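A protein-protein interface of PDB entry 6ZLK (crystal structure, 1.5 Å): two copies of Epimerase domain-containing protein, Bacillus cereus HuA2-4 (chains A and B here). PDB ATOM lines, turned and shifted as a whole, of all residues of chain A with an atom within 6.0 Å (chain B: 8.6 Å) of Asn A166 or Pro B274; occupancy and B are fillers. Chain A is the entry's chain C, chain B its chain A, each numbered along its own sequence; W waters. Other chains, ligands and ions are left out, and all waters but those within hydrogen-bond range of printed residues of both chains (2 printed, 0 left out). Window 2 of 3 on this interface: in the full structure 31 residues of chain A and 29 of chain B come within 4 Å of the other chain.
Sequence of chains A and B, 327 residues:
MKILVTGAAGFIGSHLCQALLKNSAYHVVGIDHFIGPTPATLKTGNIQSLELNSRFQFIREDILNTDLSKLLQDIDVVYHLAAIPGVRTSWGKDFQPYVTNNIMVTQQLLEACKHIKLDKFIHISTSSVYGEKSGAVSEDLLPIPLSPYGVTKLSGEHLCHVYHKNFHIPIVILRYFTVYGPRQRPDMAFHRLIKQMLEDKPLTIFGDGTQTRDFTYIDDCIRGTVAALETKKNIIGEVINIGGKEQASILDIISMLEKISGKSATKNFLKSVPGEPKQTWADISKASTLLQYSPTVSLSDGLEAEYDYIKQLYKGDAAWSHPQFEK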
ATOM      1  N   HIS A 161     -14.479  -3.599  19.581  1.00  0.00           N
ATOM      2  CA  HIS A 161     -13.762  -2.682  18.669  1.00  0.00           C
ATOM      3  C   HIS A 161     -14.726  -1.600  18.165  1.00  0.00           C
ATOM      4  O   HIS A 161     -14.319  -0.451  18.085  1.00  0.00           O
ATOM      5  CB  HIS A 161     -13.108  -3.462  17.552  1.00  0.00           C
ATOM      6  CG  HIS A 161     -12.006  -4.328  18.046  1.00  0.00           C
ATOM      7  ND1 HIS A 161     -10.868  -3.788  18.623  1.00  0.00           N
ATOM      8  CD2 HIS A 161     -11.808  -5.654  17.927  1.00  0.00           C
ATOM      9  CE1 HIS A 161     -10.051  -4.810  18.933  1.00  0.00           C
ATOM     10  NE2 HIS A 161     -10.596  -5.939  18.479  1.00  0.00           N
ATOM     11  N   VAL A 162     -15.969  -1.953  17.851  1.00  0.00           N
ATOM     12  CA  VAL A 162     -16.929  -0.933  17.349  1.00  0.00           C
ATOM     13  C   VAL A 162     -17.116   0.159  18.411  1.00  0.00           C
ATOM     14  O   VAL A 162     -17.111   1.355  18.051  1.00  0.00           O
ATOM     15  CB  VAL A 162     -18.247  -1.596  16.953  1.00  0.00           C
ATOM     16  CG1 VAL A 162     -19.348  -0.586  16.774  1.00  0.00           C
ATOM     17  CG2 VAL A 162     -18.057  -2.410  15.672  1.00  0.00           C
ATOM     18  N   TYR A 163     -17.330  -0.214  19.663  1.00  0.00           N
ATOM     19  CA  TYR A 163     -17.672   0.741  20.725  1.00  0.00           C
ATOM     20  C   TYR A 163     -16.425   1.540  21.105  1.00  0.00           C
ATOM     21  O   TYR A 163     -16.503   2.685  21.559  1.00  0.00           O
ATOM     22  CB  TYR A 163     -18.453   0.055  21.848  1.00  0.00           C
ATOM     23  CG  TYR A 163     -19.894  -0.170  21.494  1.00  0.00           C
ATOM     24  CD1 TYR A 163     -20.278  -1.265  20.729  1.00  0.00           C
ATOM     25  CD2 TYR A 163     -20.863   0.722  21.898  1.00  0.00           C
ATOM     26  CE1 TYR A 163     -21.584  -1.467  20.340  1.00  0.00           C
ATOM     27  CE2 TYR A 163     -22.186   0.525  21.550  1.00  0.00           C
ATOM     28  CZ  TYR A 163     -22.531  -0.542  20.744  1.00  0.00           C
ATOM     29  OH  TYR A 163     -23.824  -0.746  20.386  1.00  0.00           O
ATOM     30  N   HIS A 164     -15.257   0.899  21.065  1.00  0.00           N
ATOM     31  CA  HIS A 164     -13.963   1.546  21.305  1.00  0.00           C
ATOM     32  C   HIS A 164     -13.707   2.631  20.266  1.00  0.00           C
ATOM     33  O   HIS A 164     -13.449   3.802  20.645  1.00  0.00           O
ATOM     34  CB  HIS A 164     -12.867   0.501  21.338  1.00  0.00           C
ATOM     35  CG  HIS A 164     -11.530   1.135  21.454  1.00  0.00           C
ATOM     36  ND1 HIS A 164     -10.495   0.814  20.627  1.00  0.00           N
ATOM     37  CD2 HIS A 164     -11.109   2.119  22.267  1.00  0.00           C
ATOM     38  CE1 HIS A 164      -9.440   1.538  20.969  1.00  0.00           C
ATOM     39  NE2 HIS A 164      -9.793   2.357  21.967  1.00  0.00           N
ATOM     40  N   LYS A 165     -13.834   2.292  18.985  1.00  0.00           N
ATOM     41  CA  LYS A 165     -13.524   3.267  17.916  1.00  0.00           C
ATOM     42  C   LYS A 165     -14.569   4.372  17.891  1.00  0.00           C
ATOM     43  O   LYS A 165     -14.184   5.504  17.712  1.00  0.00           O
ATOM     44  CB  LYS A 165     -13.376   2.555  16.583  1.00  0.00           C
ATOM     45  CG  LYS A 165     -12.165   1.633  16.548  1.00  0.00           C
ATOM     46  CD  LYS A 165     -10.882   2.362  16.877  1.00  0.00           C
ATOM     47  CE  LYS A 165      -9.643   1.649  16.371  1.00  0.00           C
ATOM     48  NZ  LYS A 165      -8.422   2.469  16.586  1.00  0.00           N
ATOM     49  N   ASN A 166     -15.835   4.098  18.098  1.00  0.00           N
ATOM     50  CA  ASN A 166     -16.873   5.152  17.914  1.00  0.00           C
ATOM     51  C   ASN A 166     -17.092   5.940  19.214  1.00  0.00           C
ATOM     52  O   ASN A 166     -17.389   7.136  19.141  1.00  0.00           O
ATOM     53  CB  ASN A 166     -18.183   4.514  17.489  1.00  0.00           C
ATOM     54  CG  ASN A 166     -18.093   4.094  16.039  1.00  0.00           C
ATOM     55  OD1 ASN A 166     -18.139   4.957  15.154  1.00  0.00           O
ATOM     56  ND2 ASN A 166     -17.899   2.804  15.790  1.00  0.00           N
ATOM     57  N   PHE A 167     -16.994   5.309  20.377  1.00  0.00           N
ATOM     58  CA  PHE A 167     -17.389   5.946  21.673  1.00  0.00           C
ATOM     59  C   PHE A 167     -16.268   5.965  22.709  1.00  0.00           C
ATOM     60  O   PHE A 167     -16.505   6.487  23.805  1.00  0.00           O
ATOM     61  CB  PHE A 167     -18.647   5.301  22.215  1.00  0.00           C
ATOM     62  CG  PHE A 167     -19.747   5.257  21.193  1.00  0.00           C
ATOM     63  CD1 PHE A 167     -20.343   6.424  20.732  1.00  0.00           C
ATOM     64  CD2 PHE A 167     -20.195   4.043  20.709  1.00  0.00           C
ATOM     65  CE1 PHE A 167     -21.363   6.361  19.800  1.00  0.00           C
ATOM     66  CE2 PHE A 167     -21.223   3.988  19.790  1.00  0.00           C
ATOM     67  CZ  PHE A 167     -21.796   5.138  19.327  1.00  0.00           C
ATOM     68  N   HIS A 168     -15.089   5.525  22.332  1.00  0.00           N
ATOM     69  CA  HIS A 168     -13.856   5.567  23.170  1.00  0.00           C
ATOM     70  C   HIS A 168     -14.032   4.734  24.440  1.00  0.00           C
ATOM     71  O   HIS A 168     -13.297   5.041  25.435  1.00  0.00           O
ATOM     72  CB  HIS A 168     -13.457   7.017  23.523  1.00  0.00           C
ATOM     73  CG  HIS A 168     -13.484   7.881  22.315  1.00  0.00           C
ATOM     74  ND1 HIS A 168     -14.613   8.614  21.957  1.00  0.00           N
ATOM     75  CD2 HIS A 168     -12.611   7.992  21.292  1.00  0.00           C
ATOM     76  CE1 HIS A 168     -14.400   9.190  20.786  1.00  0.00           C
ATOM     77  NE2 HIS A 168     -13.171   8.839  20.371  1.00  0.00           N
ATOM     78  N   GLY B  86     -28.058  -1.581   6.698  1.00  0.00           N
ATOM     79  CA  GLY B  86     -28.168  -0.183   7.155  1.00  0.00           C
ATOM     80  C   GLY B  86     -27.168   0.021   8.265  1.00  0.00           C
ATOM     81  O   GLY B  86     -27.412  -0.448   9.428  1.00  0.00           O
ATOM     82  N   VAL B  87     -26.051   0.635   7.900  1.00  0.00           N
ATOM     83  CA  VAL B  87     -24.935   0.887   8.829  1.00  0.00           C
ATOM     84  C   VAL B  87     -25.478   1.765   9.968  1.00  0.00           C
ATOM     85  O   VAL B  87     -25.110   1.579  11.103  1.00  0.00           O
ATOM     86  CB  VAL B  87     -23.767   1.521   8.052  1.00  0.00           C
ATOM     87  CG1 VAL B  87     -22.718   2.131   8.960  1.00  0.00           C
ATOM     88  CG2 VAL B  87     -23.154   0.529   7.067  1.00  0.00           C
ATOM     89  N   ARG B  88     -26.294   2.766   9.649  1.00  0.00           N
ATOM     90  CA  ARG B  88     -26.475   3.909  10.572  1.00  0.00           C
ATOM     91  C   ARG B  88     -27.568   3.609  11.593  1.00  0.00           C
ATOM     92  O   ARG B  88     -27.695   4.376  12.568  1.00  0.00           O
ATOM     93  CB  ARG B  88     -26.777   5.168   9.744  1.00  0.00           C
ATOM     94  CG  ARG B  88     -25.590   5.606   8.894  1.00  0.00           C
ATOM     95  CD  ARG B  88     -25.894   6.837   8.034  1.00  0.00           C
ATOM     96  NE  ARG B  88     -26.857   6.603   6.969  1.00  0.00           N
ATOM     97  CZ  ARG B  88     -26.571   6.040   5.790  1.00  0.00           C
ATOM     98  NH1 ARG B  88     -27.520   5.862   4.881  1.00  0.00           N
ATOM     99  NH2 ARG B  88     -25.320   5.681   5.531  1.00  0.00           N
ATOM    100  N   THR B  89     -28.400   2.600  11.381  1.00  0.00           N
ATOM    101  CA  THR B  89     -29.561   2.297  12.251  1.00  0.00           C
ATOM    102  C   THR B  89     -29.359   0.982  13.003  1.00  0.00           C
ATOM    103  O   THR B  89     -30.348   0.324  13.285  1.00  0.00           O
ATOM    104  CB  THR B  89     -30.836   2.276  11.405  1.00  0.00           C
ATOM    105  OG1 THR B  89     -30.664   1.262  10.408  1.00  0.00           O
ATOM    106  CG2 THR B  89     -31.090   3.633  10.786  1.00  0.00           C
ATOM    107  N   SER B  90     -28.112   0.611  13.345  1.00  0.00           N
ATOM    108  CA  SER B  90     -27.788  -0.714  13.944  1.00  0.00           C
ATOM    109  C   SER B  90     -27.399  -0.541  15.414  1.00  0.00           C
ATOM    110  O   SER B  90     -26.903  -1.535  16.014  1.00  0.00           O
ATOM    111  CB  SER B  90     -26.692  -1.459  13.171  1.00  0.00           C
ATOM    112  OG  SER B  90     -25.469  -0.745  13.049  1.00  0.00           O
ATOM    113  N   TRP B  91     -27.700   0.605  16.021  1.00  0.00           N
ATOM    114  CA  TRP B  91     -27.297   0.938  17.417  1.00  0.00           C
ATOM    115  C   TRP B  91     -28.412   0.637  18.399  1.00  0.00           C
ATOM    116  O   TRP B  91     -29.583   0.566  18.000  1.00  0.00           O
ATOM    117  CB  TRP B  91     -26.841   2.396  17.547  1.00  0.00           C
ATOM    118  CG  TRP B  91     -25.729   2.750  16.633  1.00  0.00           C
ATOM    119  CD1 TRP B  91     -25.851   3.469  15.486  1.00  0.00           C
ATOM    120  CD2 TRP B  91     -24.336   2.450  16.773  1.00  0.00           C
ATOM    121  NE1 TRP B  91     -24.641   3.555  14.870  1.00  0.00           N
ATOM    122  CE2 TRP B  91     -23.689   2.943  15.626  1.00  0.00           C
ATOM    123  CE3 TRP B  91     -23.568   1.790  17.729  1.00  0.00           C
ATOM    124  CZ2 TRP B  91     -22.316   2.874  15.454  1.00  0.00           C
ATOM    125  CZ3 TRP B  91     -22.218   1.680  17.540  1.00  0.00           C
ATOM    126  CH2 TRP B  91     -21.594   2.244  16.421  1.00  0.00           C
ATOM    127  N   ILE B 144     -12.180  -5.510  10.420  1.00  0.00           N
ATOM    128  CA  ILE B 144     -12.535  -4.934  11.736  1.00  0.00           C
ATOM    129  C   ILE B 144     -13.678  -3.969  11.506  1.00  0.00           C
ATOM    130  O   ILE B 144     -13.510  -2.788  11.248  1.00  0.00           O
ATOM    131  CB  ILE B 144     -11.363  -4.266  12.455  1.00  0.00           C
ATOM    132  CG1 ILE B 144     -10.084  -5.105  12.466  1.00  0.00           C
ATOM    133  CG2 ILE B 144     -11.836  -3.949  13.869  1.00  0.00           C
ATOM    134  N   PRO B 145     -14.916  -4.485  11.560  1.00  0.00           N
ATOM    135  CA  PRO B 145     -16.054  -3.615  11.286  1.00  0.00           C
ATOM    136  C   PRO B 145     -16.113  -2.386  12.196  1.00  0.00           C
ATOM    137  O   PRO B 145     -15.635  -2.417  13.351  1.00  0.00           O
ATOM    138  CB  PRO B 145     -17.236  -4.543  11.593  1.00  0.00           C
ATOM    139  CG  PRO B 145     -16.740  -5.928  11.422  1.00  0.00           C
ATOM    140  CD  PRO B 145     -15.265  -5.880  11.771  1.00  0.00           C
ATOM    141  N   LEU B 146     -16.655  -1.299  11.658  1.00  0.00           N
ATOM    142  CA  LEU B 146     -16.859  -0.037  12.392  1.00  0.00           C
ATOM    143  C   LEU B 146     -18.297   0.096  12.902  1.00  0.00           C
ATOM    144  O   LEU B 146     -18.582   1.015  13.742  1.00  0.00           O
ATOM    145  CB  LEU B 146     -16.581   1.124  11.441  1.00  0.00           C
ATOM    146  CG  LEU B 146     -15.232   1.807  11.538  1.00  0.00           C
ATOM    147  CD1 LEU B 146     -15.242   2.978  10.532  1.00  0.00           C
ATOM    148  CD2 LEU B 146     -14.979   2.280  12.984  1.00  0.00           C
ATOM    149  N   SER B 147     -19.208  -0.762  12.434  1.00  0.00           N
ATOM    150  CA  SER B 147     -20.633  -0.702  12.828  1.00  0.00           C
ATOM    151  C   SER B 147     -21.117  -2.047  13.345  1.00  0.00           C
ATOM    152  O   SER B 147     -20.660  -3.097  12.893  1.00  0.00           O
ATOM    153  CB  SER B 147     -21.530  -0.283  11.660  1.00  0.00           C
ATOM    154  OG  SER B 147     -21.439  -1.232  10.601  1.00  0.00           O
ATOM    155  N   PRO B 148     -22.135  -2.038  14.237  1.00  0.00           N
ATOM    156  CA  PRO B 148     -22.812  -3.249  14.649  1.00  0.00           C
ATOM    157  C   PRO B 148     -23.391  -4.043  13.476  1.00  0.00           C
ATOM    158  O   PRO B 148     -23.292  -5.223  13.445  1.00  0.00           O
ATOM    159  CB  PRO B 148     -23.889  -2.773  15.630  1.00  0.00           C
ATOM    160  CG  PRO B 148     -23.368  -1.418  16.115  1.00  0.00           C
ATOM    161  CD  PRO B 148     -22.673  -0.845  14.915  1.00  0.00           C
ATOM    162  N   PHE B 206     -24.140  13.803   5.629  1.00  0.00           N
ATOM    163  CA  PHE B 206     -23.585  13.395   6.934  1.00  0.00           C
ATOM    164  C   PHE B 206     -22.098  13.704   6.901  1.00  0.00           C
ATOM    165  O   PHE B 206     -21.380  13.311   5.959  1.00  0.00           O
ATOM    166  CB  PHE B 206     -23.987  11.945   7.264  1.00  0.00           C
ATOM    167  CG  PHE B 206     -25.462  11.682   7.189  1.00  0.00           C
ATOM    168  CD1 PHE B 206     -26.385  12.694   7.454  1.00  0.00           C
ATOM    169  CD2 PHE B 206     -25.953  10.443   6.833  1.00  0.00           C
ATOM    170  CE1 PHE B 206     -27.749  12.457   7.388  1.00  0.00           C
ATOM    171  CE2 PHE B 206     -27.311  10.203   6.796  1.00  0.00           C
ATOM    172  CZ  PHE B 206     -28.212  11.201   7.066  1.00  0.00           C
ATOM    173  N   LYS B 271     -24.239  16.365  11.483  1.00  0.00           N
ATOM    174  CA  LYS B 271     -23.160  15.709  12.246  1.00  0.00           C
ATOM    175  C   LYS B 271     -22.904  14.337  11.614  1.00  0.00           C
ATOM    176  O   LYS B 271     -23.840  13.598  11.233  1.00  0.00           O
ATOM    177  CB  LYS B 271     -23.567  15.685  13.722  1.00  0.00           C
ATOM    178  CG  LYS B 271     -22.551  15.091  14.685  1.00  0.00           C
ATOM    179  CD  LYS B 271     -21.287  15.908  14.838  1.00  0.00           C
ATOM    180  CE  LYS B 271     -20.242  15.183  15.667  1.00  0.00           C
ATOM    181  NZ  LYS B 271     -19.598  14.069  14.919  1.00  0.00           N
ATOM    182  N   SER B 272     -21.636  13.994  11.451  1.00  0.00           N
ATOM    183  CA  SER B 272     -21.291  12.651  10.943  1.00  0.00           C
ATOM    184  C   SER B 272     -21.896  11.635  11.924  1.00  0.00           C
ATOM    185  O   SER B 272     -22.070  11.964  13.117  1.00  0.00           O
ATOM    186  CB  SER B 272     -19.811  12.512  10.742  1.00  0.00           C
ATOM    187  OG  SER B 272     -19.178  12.678  11.989  1.00  0.00           O
ATOM    188  N   VAL B 273     -22.241  10.480  11.392  1.00  0.00           N
ATOM    189  CA  VAL B 273     -22.952   9.369  12.078  1.00  0.00           C
ATOM    190  C   VAL B 273     -21.868   8.388  12.506  1.00  0.00           C
ATOM    191  O   VAL B 273     -20.928   8.148  11.742  1.00  0.00           O
ATOM    192  CB  VAL B 273     -23.963   8.722  11.110  1.00  0.00           C
ATOM    193  CG1 VAL B 273     -25.018   7.951  11.855  1.00  0.00           C
ATOM    194  CG2 VAL B 273     -24.642   9.746  10.221  1.00  0.00           C
ATOM    195  N   PRO B 274     -21.916   7.837  13.738  1.00  0.00           N
ATOM    196  CA  PRO B 274     -20.984   6.779  14.106  1.00  0.00           C
ATOM    197  C   PRO B 274     -21.166   5.534  13.233  1.00  0.00           C
ATOM    198  O   PRO B 274     -22.247   5.250  12.730  1.00  0.00           O
ATOM    199  CB  PRO B 274     -21.287   6.432  15.573  1.00  0.00           C
ATOM    200  CG  PRO B 274     -22.574   7.123  15.905  1.00  0.00           C
ATOM    201  CD  PRO B 274     -22.822   8.176  14.844  1.00  0.00           C
ATOM    202  N   GLY B 275     -20.080   4.800  13.063  1.00  0.00           N
ATOM    203  CA  GLY B 275     -20.162   3.496  12.387  1.00  0.00           C
ATOM    204  C   GLY B 275     -19.778   3.546  10.931  1.00  0.00           C
ATOM    205  O   GLY B 275     -19.751   2.483  10.329  1.00  0.00           O
ATOM    206  N   GLU B 276     -19.518   4.724  10.373  1.00  0.00           N
ATOM    207  CA  GLU B 276     -19.333   4.801   8.898  1.00  0.00           C
ATOM    208  C   GLU B 276     -17.882   5.097   8.614  1.00  0.00           C
ATOM    209  O   GLU B 276     -17.324   6.042   9.178  1.00  0.00           O
ATOM    210  CB  GLU B 276     -20.146   5.918   8.290  1.00  0.00           C
ATOM    211  CG  GLU B 276     -21.591   5.888   8.644  1.00  0.00           C
ATOM    212  CD  GLU B 276     -22.354   6.666   7.594  1.00  0.00           C
ATOM    213  OE1 GLU B 276     -22.380   7.925   7.692  1.00  0.00           O
ATOM    214  OE2 GLU B 276     -22.892   6.011   6.707  1.00  0.00           O
ATOM    215  N   PRO B 277     -17.236   4.348   7.695  1.00  0.00           N
ATOM    216  CA  PRO B 277     -15.888   4.672   7.271  1.00  0.00           C
ATOM    217  C   PRO B 277     -15.852   5.923   6.380  1.00  0.00           C
ATOM    218  O   PRO B 277     -16.843   6.255   5.711  1.00  0.00           O
ATOM    219  CB  PRO B 277     -15.493   3.446   6.430  1.00  0.00           C
ATOM    220  CG  PRO B 277     -16.800   2.971   5.852  1.00  0.00           C
ATOM    221  CD  PRO B 277     -17.808   3.182   6.965  1.00  0.00           C
HETATM  222  O   HOH W   1     -25.568  -1.840  18.513  1.00  0.00           O
HETATM  223  O   HOH W   2     -14.094  -0.617  14.946  1.00  0.00           O
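Water W1 lies within hydrogen-bond range of the side-chain hydroxyl of Tyr A163 (2.8 Å) and the backbone carbonyl oxygen of Ser B90 (2.8 Å). Water W2 lies within hydrogen-bond range of O of Pro B145 (2.9 Å) and O of His A161 (3.2 Å).
The backbone carbonyl oxygen (O) of Val A162 sits at hydrogen-bond distance from the side-chain amide nitrogen (ND2) of Asn A166 (2.8 Å). N of His A168 is in hydrogen-bond range of O of Tyr A163 (3.3 Å).
Hydrophobic or aromatic side chains of chain B that line the printed part of chain A: Trp B91, Ile B144, Leu B146, Pro B148 and Pro B274. Of the 8 printed residues of chain A, 6 touch a printed residue of chain B. Hydrophobic or aromatic side chains of chain A that line the printed part of chain B: His A161, Val A162, Tyr A163 and Phe A167. Among the printed residues, 13 pairs touch across the chains. Among the printed residues, no Asp or Glu carboxylate lies within 4 Å of a Lys or Arg side-chain nitrogen of the other chain.
Printed residues of chain B within 4 Å of His A161: Ile B144 (3.9 Å). Of the printed residues of chain B, Val A162 touches Trp B91 (3.6 Å), Pro B145 (3.4 Å), Leu B146 (3.5 Å), Ser B147 (3.8 Å) and Pro B148 (3.8 Å). Asn A166 touches just these residues of chain B: Trp B91 (3.8 Å), Leu B146 (2.8 Å), Pro B274 (3.5 Å) and Gly B275 (2.9 Å). Gly B86 touches none of the printed residues of chain A. Arg B88 touches none of the printed residues of chain A. Of the printed residues of chain A, Trp B91 touches Val A162 (3.6 Å), Tyr A163 (3.7 Å), Asn A166 (3.8 Å) and Phe A167 (3.4 Å). Printed residues of chain A within 4 Å of Ser B147: Val A162. Of the printed residues of chain A, Pro B274 touches Asn A166 (3.5 Å). The nearest printed residue of chain B that does not touch Lys A165 is Ile B144 (6.2 Å).
OD1 of Asn A166 is in hydrogen-bond range of N of Gly B275. The backbone carbonyl oxygen (O) of Leu B146 is in hydrogen-bond range of the side-chain amide nitrogen (ND2) of Asn A166, at 2.8 Å.
No position is printed for both chains. Of the 13 pairs that touch across the chains among the printed residues, none has its exchanged pair printed and touching as well.
Among the printed residues, merely in contact across the chains: His A161 with Ile B144 (3.9 Å), Val A162 with Trp B91 (3.6 Å), Val A162 with Pro B145 (3.4 Å), Val A162 with Leu B146 (3.5 Å), Val A162 with Ser B147 (3.8 Å), Val A162 with Pro B148 (3.8 Å), Tyr A163 with Trp B91 (3.7 Å), Lys A165 with Leu B146 (3.9 Å), Asn A166 with Trp B91 (3.8 Å), Asn A166 with Pro B274 (3.5 Å) and Phe A167 with Trp B91 (3.4 Å).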
